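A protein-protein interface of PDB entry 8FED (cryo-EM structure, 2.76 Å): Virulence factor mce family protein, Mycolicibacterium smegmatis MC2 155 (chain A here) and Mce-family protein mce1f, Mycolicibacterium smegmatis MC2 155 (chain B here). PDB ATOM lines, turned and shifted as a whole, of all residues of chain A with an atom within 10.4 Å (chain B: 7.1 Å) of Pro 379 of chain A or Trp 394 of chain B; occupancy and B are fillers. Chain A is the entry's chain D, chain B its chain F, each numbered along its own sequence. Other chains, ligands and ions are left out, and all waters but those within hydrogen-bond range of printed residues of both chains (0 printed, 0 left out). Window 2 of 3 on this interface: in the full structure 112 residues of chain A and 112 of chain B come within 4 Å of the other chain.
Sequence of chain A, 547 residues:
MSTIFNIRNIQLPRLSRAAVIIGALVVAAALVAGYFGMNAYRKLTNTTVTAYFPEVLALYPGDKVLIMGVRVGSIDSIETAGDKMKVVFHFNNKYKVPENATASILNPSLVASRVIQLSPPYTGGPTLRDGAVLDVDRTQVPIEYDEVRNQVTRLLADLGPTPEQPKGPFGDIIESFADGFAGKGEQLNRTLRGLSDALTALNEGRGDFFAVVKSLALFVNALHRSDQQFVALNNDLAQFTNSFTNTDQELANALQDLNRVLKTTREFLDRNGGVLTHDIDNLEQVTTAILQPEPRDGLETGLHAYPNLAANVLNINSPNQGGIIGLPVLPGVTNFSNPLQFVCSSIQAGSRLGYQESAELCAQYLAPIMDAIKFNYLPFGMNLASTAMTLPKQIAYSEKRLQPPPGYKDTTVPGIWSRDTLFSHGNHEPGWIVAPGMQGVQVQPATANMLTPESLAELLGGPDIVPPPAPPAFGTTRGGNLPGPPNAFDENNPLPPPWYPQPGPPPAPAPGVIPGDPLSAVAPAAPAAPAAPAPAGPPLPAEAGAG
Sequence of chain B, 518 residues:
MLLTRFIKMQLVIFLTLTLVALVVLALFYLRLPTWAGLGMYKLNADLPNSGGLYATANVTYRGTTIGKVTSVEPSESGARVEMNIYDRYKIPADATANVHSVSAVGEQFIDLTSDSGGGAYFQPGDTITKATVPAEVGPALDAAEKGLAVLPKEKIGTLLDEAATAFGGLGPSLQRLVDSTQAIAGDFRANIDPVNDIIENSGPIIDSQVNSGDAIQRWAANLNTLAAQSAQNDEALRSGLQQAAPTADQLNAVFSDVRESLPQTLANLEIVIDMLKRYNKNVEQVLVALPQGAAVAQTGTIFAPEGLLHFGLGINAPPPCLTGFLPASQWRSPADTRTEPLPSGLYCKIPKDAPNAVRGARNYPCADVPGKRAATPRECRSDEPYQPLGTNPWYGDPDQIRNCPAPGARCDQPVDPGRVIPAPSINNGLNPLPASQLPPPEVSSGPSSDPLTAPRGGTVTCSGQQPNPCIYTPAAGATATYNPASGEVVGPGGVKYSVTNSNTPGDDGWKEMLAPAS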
ATOM      1  N   PHE A 375      -5.406  26.988 -18.406  1.00  0.00           N
ATOM      2  CA  PHE A 375      -5.445  26.760 -19.846  1.00  0.00           C
ATOM      3  C   PHE A 375      -4.188  27.304 -20.516  1.00  0.00           C
ATOM      4  O   PHE A 375      -3.507  28.166 -19.966  1.00  0.00           O
ATOM      5  CB  PHE A 375      -6.698  27.398 -20.456  1.00  0.00           C
ATOM      6  CG  PHE A 375      -6.774  28.889 -20.281  1.00  0.00           C
ATOM      7  CD1 PHE A 375      -7.270  29.441 -19.112  1.00  0.00           C
ATOM      8  CD2 PHE A 375      -6.362  29.739 -21.292  1.00  0.00           C
ATOM      9  CE1 PHE A 375      -7.344  30.812 -18.951  1.00  0.00           C
ATOM     10  CE2 PHE A 375      -6.433  31.110 -21.139  1.00  0.00           C
ATOM     11  CZ  PHE A 375      -6.925  31.647 -19.966  1.00  0.00           C
ATOM     12  N   ASN A 376      -3.882  26.784 -21.708  1.00  0.00           N
ATOM     13  CA  ASN A 376      -2.631  27.135 -22.371  1.00  0.00           C
ATOM     14  C   ASN A 376      -2.632  28.584 -22.846  1.00  0.00           C
ATOM     15  O   ASN A 376      -1.687  29.333 -22.574  1.00  0.00           O
ATOM     16  CB  ASN A 376      -2.370  26.183 -23.537  1.00  0.00           C
ATOM     17  CG  ASN A 376      -2.137  24.757 -23.082  1.00  0.00           C
ATOM     18  OD1 ASN A 376      -1.756  24.515 -21.938  1.00  0.00           O
ATOM     19  ND2 ASN A 376      -2.359  23.805 -23.980  1.00  0.00           N
ATOM     20  N   TYR A 377      -3.686  28.999 -23.543  1.00  0.00           N
ATOM     21  CA  TYR A 377      -3.784  30.360 -24.068  1.00  0.00           C
ATOM     22  C   TYR A 377      -5.230  30.620 -24.481  1.00  0.00           C
ATOM     23  O   TYR A 377      -6.093  29.743 -24.389  1.00  0.00           O
ATOM     24  CB  TYR A 377      -2.813  30.588 -25.229  1.00  0.00           C
ATOM     25  CG  TYR A 377      -2.921  29.584 -26.353  1.00  0.00           C
ATOM     26  CD1 TYR A 377      -2.156  28.426 -26.350  1.00  0.00           C
ATOM     27  CD2 TYR A 377      -3.768  29.804 -27.427  1.00  0.00           C
ATOM     28  CE1 TYR A 377      -2.244  27.512 -27.377  1.00  0.00           C
ATOM     29  CE2 TYR A 377      -3.864  28.897 -28.457  1.00  0.00           C
ATOM     30  CZ  TYR A 377      -3.099  27.754 -28.429  1.00  0.00           C
ATOM     31  OH  TYR A 377      -3.194  26.848 -29.459  1.00  0.00           O
ATOM     32  N   LEU A 378      -5.480  31.843 -24.944  1.00  0.00           N
ATOM     33  CA  LEU A 378      -6.835  32.265 -25.267  1.00  0.00           C
ATOM     34  C   LEU A 378      -7.338  31.562 -26.525  1.00  0.00           C
ATOM     35  O   LEU A 378      -6.567  31.334 -27.463  1.00  0.00           O
ATOM     36  CB  LEU A 378      -6.888  33.779 -25.466  1.00  0.00           C
ATOM     37  CG  LEU A 378      -6.507  34.645 -24.265  1.00  0.00           C
ATOM     38  CD1 LEU A 378      -6.526  36.113 -24.647  1.00  0.00           C
ATOM     39  CD2 LEU A 378      -7.443  34.381 -23.100  1.00  0.00           C
ATOM     40  N   PRO A 379      -8.626  31.208 -26.578  1.00  0.00           N
ATOM     41  CA  PRO A 379      -9.161  30.531 -27.770  1.00  0.00           C
ATOM     42  C   PRO A 379      -9.175  31.394 -29.017  1.00  0.00           C
ATOM     43  O   PRO A 379      -9.268  30.848 -30.122  1.00  0.00           O
ATOM     44  CB  PRO A 379     -10.588  30.147 -27.351  1.00  0.00           C
ATOM     45  CG  PRO A 379     -10.605  30.254 -25.856  1.00  0.00           C
ATOM     46  CD  PRO A 379      -9.638  31.336 -25.516  1.00  0.00           C
ATOM     47  N   PHE A 380      -9.097  32.715 -28.884  1.00  0.00           N
ATOM     48  CA  PHE A 380      -9.256  33.630 -30.005  1.00  0.00           C
ATOM     49  C   PHE A 380      -8.007  34.483 -30.171  1.00  0.00           C
ATOM     50  O   PHE A 380      -7.385  34.891 -29.185  1.00  0.00           O
ATOM     51  CB  PHE A 380     -10.486  34.525 -29.811  1.00  0.00           C
ATOM     52  CG  PHE A 380     -10.710  34.952 -28.385  1.00  0.00           C
ATOM     53  CD1 PHE A 380      -9.976  35.985 -27.828  1.00  0.00           C
ATOM     54  CD2 PHE A 380     -11.664  34.320 -27.604  1.00  0.00           C
ATOM     55  CE1 PHE A 380     -10.184  36.377 -26.520  1.00  0.00           C
ATOM     56  CE2 PHE A 380     -11.877  34.710 -26.294  1.00  0.00           C
ATOM     57  CZ  PHE A 380     -11.136  35.739 -25.753  1.00  0.00           C
ATOM     58  N   GLY A 381      -7.646  34.744 -31.419  1.00  0.00           N
ATOM     59  CA  GLY A 381      -6.497  35.578 -31.717  1.00  0.00           C
ATOM     60  C   GLY A 381      -6.782  36.471 -32.904  1.00  0.00           C
ATOM     61  O   GLY A 381      -7.568  36.129 -33.790  1.00  0.00           O
ATOM     62  N   MET A 382      -6.125  37.628 -32.916  1.00  0.00           N
ATOM     63  CA  MET A 382      -6.383  38.650 -33.917  1.00  0.00           C
ATOM     64  C   MET A 382      -5.076  39.139 -34.524  1.00  0.00           C
ATOM     65  O   MET A 382      -4.026  39.132 -33.876  1.00  0.00           O
ATOM     66  CB  MET A 382      -7.153  39.835 -33.316  1.00  0.00           C
ATOM     67  CG  MET A 382      -7.963  40.630 -34.326  1.00  0.00           C
ATOM     68  SD  MET A 382      -9.046  41.842 -33.551  1.00  0.00           S
ATOM     69  CE  MET A 382     -10.260  42.081 -34.847  1.00  0.00           C
ATOM     70  N   ASN B 316      -2.008  36.484 -29.885  1.00  0.00           N
ATOM     71  CA  ASN B 316      -2.353  35.098 -30.209  1.00  0.00           C
ATOM     72  C   ASN B 316      -2.703  34.912 -31.683  1.00  0.00           C
ATOM     73  O   ASN B 316      -3.554  34.088 -32.024  1.00  0.00           O
ATOM     74  CB  ASN B 316      -3.502  34.588 -29.333  1.00  0.00           C
ATOM     75  CG  ASN B 316      -3.071  34.308 -27.912  1.00  0.00           C
ATOM     76  OD1 ASN B 316      -1.932  33.918 -27.663  1.00  0.00           O
ATOM     77  ND2 ASN B 316      -3.982  34.507 -26.969  1.00  0.00           N
ATOM     78  N   THR B 391      -1.279  17.249 -31.506  1.00  0.00           N
ATOM     79  CA  THR B 391      -1.705  18.595 -31.866  1.00  0.00           C
ATOM     80  C   THR B 391      -1.787  19.466 -30.616  1.00  0.00           C
ATOM     81  O   THR B 391      -2.178  19.002 -29.542  1.00  0.00           O
ATOM     82  CB  THR B 391      -3.061  18.552 -32.574  1.00  0.00           C
ATOM     83  OG1 THR B 391      -3.024  17.570 -33.617  1.00  0.00           O
ATOM     84  CG2 THR B 391      -3.392  19.904 -33.193  1.00  0.00           C
ATOM     85  N   ASN B 392      -1.406  20.729 -30.761  1.00  0.00           N
ATOM     86  CA  ASN B 392      -1.341  21.636 -29.624  1.00  0.00           C
ATOM     87  C   ASN B 392      -2.742  22.085 -29.228  1.00  0.00           C
ATOM     88  O   ASN B 392      -3.444  22.687 -30.050  1.00  0.00           O
ATOM     89  CB  ASN B 392      -0.479  22.846 -29.963  1.00  0.00           C
ATOM     90  CG  ASN B 392      -0.295  23.784 -28.786  1.00  0.00           C
ATOM     91  OD1 ASN B 392      -0.501  23.405 -27.634  1.00  0.00           O
ATOM     92  ND2 ASN B 392       0.093  25.018 -29.074  1.00  0.00           N
ATOM     93  N   PRO B 393      -3.189  21.818 -28.006  1.00  0.00           N
ATOM     94  CA  PRO B 393      -4.465  22.355 -27.536  1.00  0.00           C
ATOM     95  C   PRO B 393      -4.264  23.680 -26.809  1.00  0.00           C
ATOM     96  O   PRO B 393      -3.141  24.118 -26.551  1.00  0.00           O
ATOM     97  CB  PRO B 393      -4.966  21.269 -26.567  1.00  0.00           C
ATOM     98  CG  PRO B 393      -3.781  20.319 -26.350  1.00  0.00           C
ATOM     99  CD  PRO B 393      -2.581  20.934 -27.002  1.00  0.00           C
ATOM    100  N   TRP B 394      -5.386  24.315 -26.480  1.00  0.00           N
ATOM    101  CA  TRP B 394      -5.374  25.528 -25.678  1.00  0.00           C
ATOM    102  C   TRP B 394      -5.929  25.321 -24.277  1.00  0.00           C
ATOM    103  O   TRP B 394      -5.939  26.269 -23.484  1.00  0.00           O
ATOM    104  CB  TRP B 394      -6.148  26.646 -26.387  1.00  0.00           C
ATOM    105  CG  TRP B 394      -7.578  26.322 -26.658  1.00  0.00           C
ATOM    106  CD1 TRP B 394      -8.085  25.736 -27.777  1.00  0.00           C
ATOM    107  CD2 TRP B 394      -8.693  26.573 -25.797  1.00  0.00           C
ATOM    108  NE1 TRP B 394      -9.447  25.603 -27.667  1.00  0.00           N
ATOM    109  CE2 TRP B 394      -9.845  26.110 -26.459  1.00  0.00           C
ATOM    110  CE3 TRP B 394      -8.828  27.144 -24.528  1.00  0.00           C
ATOM    111  CZ2 TRP B 394     -11.114  26.200 -25.898  1.00  0.00           C
ATOM    112  CZ3 TRP B 394     -10.088  27.231 -23.972  1.00  0.00           C
ATOM    113  CH2 TRP B 394     -11.215  26.762 -24.656  1.00  0.00           C
ATOM    114  N   TYR B 395      -6.375  24.111 -23.941  1.00  0.00           N
ATOM    115  CA  TYR B 395      -6.890  23.835 -22.605  1.00  0.00           C
ATOM    116  C   TYR B 395      -6.037  22.762 -21.937  1.00  0.00           C
ATOM    117  O   TYR B 395      -6.545  21.742 -21.463  1.00  0.00           O
ATOM    118  CB  TYR B 395      -8.367  23.427 -22.666  1.00  0.00           C
ATOM    119  CG  TYR B 395      -8.998  23.168 -21.311  1.00  0.00           C
ATOM    120  CD1 TYR B 395      -8.969  24.134 -20.315  1.00  0.00           C
ATOM    121  CD2 TYR B 395      -9.608  21.954 -21.028  1.00  0.00           C
ATOM    122  CE1 TYR B 395      -9.535  23.900 -19.077  1.00  0.00           C
ATOM    123  CE2 TYR B 395     -10.176  21.710 -19.794  1.00  0.00           C
ATOM    124  CZ  TYR B 395     -10.138  22.687 -18.823  1.00  0.00           C
ATOM    125  OH  TYR B 395     -10.706  22.447 -17.593  1.00  0.00           O
ATOM    126  N   GLY B 396      -4.727  22.968 -21.933  1.00  0.00           N
ATOM    127  CA  GLY B 396      -3.849  22.081 -21.206  1.00  0.00           C
ATOM    128  C   GLY B 396      -3.710  20.716 -21.860  1.00  0.00           C
ATOM    129  O   GLY B 396      -4.151  20.471 -22.985  1.00  0.00           O
ATOM    130  N   ASP B 397      -3.101  19.813 -21.096  1.00  0.00           N
ATOM    131  CA  ASP B 397      -2.758  18.471 -21.554  1.00  0.00           C
ATOM    132  C   ASP B 397      -2.035  18.467 -22.904  1.00  0.00           C
ATOM    133  O   ASP B 397      -2.489  17.820 -23.855  1.00  0.00           O
ATOM    134  CB  ASP B 397      -4.002  17.596 -21.610  1.00  0.00           C
ATOM    135  CG  ASP B 397      -4.692  17.474 -20.265  1.00  0.00           C
ATOM    136  OD1 ASP B 397      -5.086  18.516 -19.702  1.00  0.00           O
ATOM    137  OD2 ASP B 397      -4.844  16.336 -19.773  1.00  0.00           O
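Printed residues of chain B that touch a printed residue of chain A: Asn 316, Asn 392, Pro 393, Trp 394, Tyr 395 and Gly 396.
Hydrophobic or aromatic side chains of chain B within 4 Å of the printed part of chain A: Trp 394 and Tyr 395.
Among the printed residues, 12 pairs touch across the chains.
ND2 of Asn 376 of chain A lies close to N of Gly 396 of chain B (3.2 Å).
The backbone carbonyl oxygen (O) of Trp 394 of chain B is in hydrogen-bond range of the backbone NH (N) of Asn 376 of chain A, at 2.8 Å.
The side-chain amide nitrogen (ND2) of Asn 376 of chain A sits at hydrogen-bond distance from the backbone carbonyl oxygen (O) of Pro 393 of chain B (2.7 Å).
Among the printed residues, merely in contact across the chains: Phe 375 of chain A with Trp 394 of chain B (3.3 Å), Phe 375 of chain A with Tyr 395 of chain B (3.98 Å), Tyr 377 of chain A with Asn 392 of chain B (3.8 Å), Tyr 377 of chain A with Pro 393 of chain B (3.6 Å), Tyr 377 of chain A with Trp 394 of chain B (3.5 Å), Leu 378 of chain A with Asn 316 of chain B (3.4 Å), Pro 379 of chain A with Trp 394 of chain B (3.6 Å), Phe 380 of chain A with Asn 316 of chain B (3.9 Å) and Gly 381 of chain A with Asn 316 of chain B (3.3 Å).
Of the printed residues of chain B, Phe 375 of chain A touches Trp 394 and Tyr 395.
Printed residues of chain B within 4 Å of Pro 379 of chain A: Trp 394 (3.6 Å).
Printed residues of chain B within 4 Å of Phe 380 of chain A: Asn 316.
Printed residues of chain B within 4 Å of Gly 381 of chain A: Asn 316 (3.3 Å).
Thr 391 of chain B touches none of the printed residues of chain A.
Of the printed residues of chain A, Asn 392 of chain B touches Tyr 377 (3.8 Å).
Of chain A, only Phe 375, Asn 376, Tyr 377 and Pro 379 come within 4 Å of Trp 394 of chain B.
Of the printed residues of chain A, Tyr 395 of chain B touches Phe 375.
Gly 396 of chain B touches one residue of chain A.
Asp 397 of chain B touches none of the printed residues of chain A.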
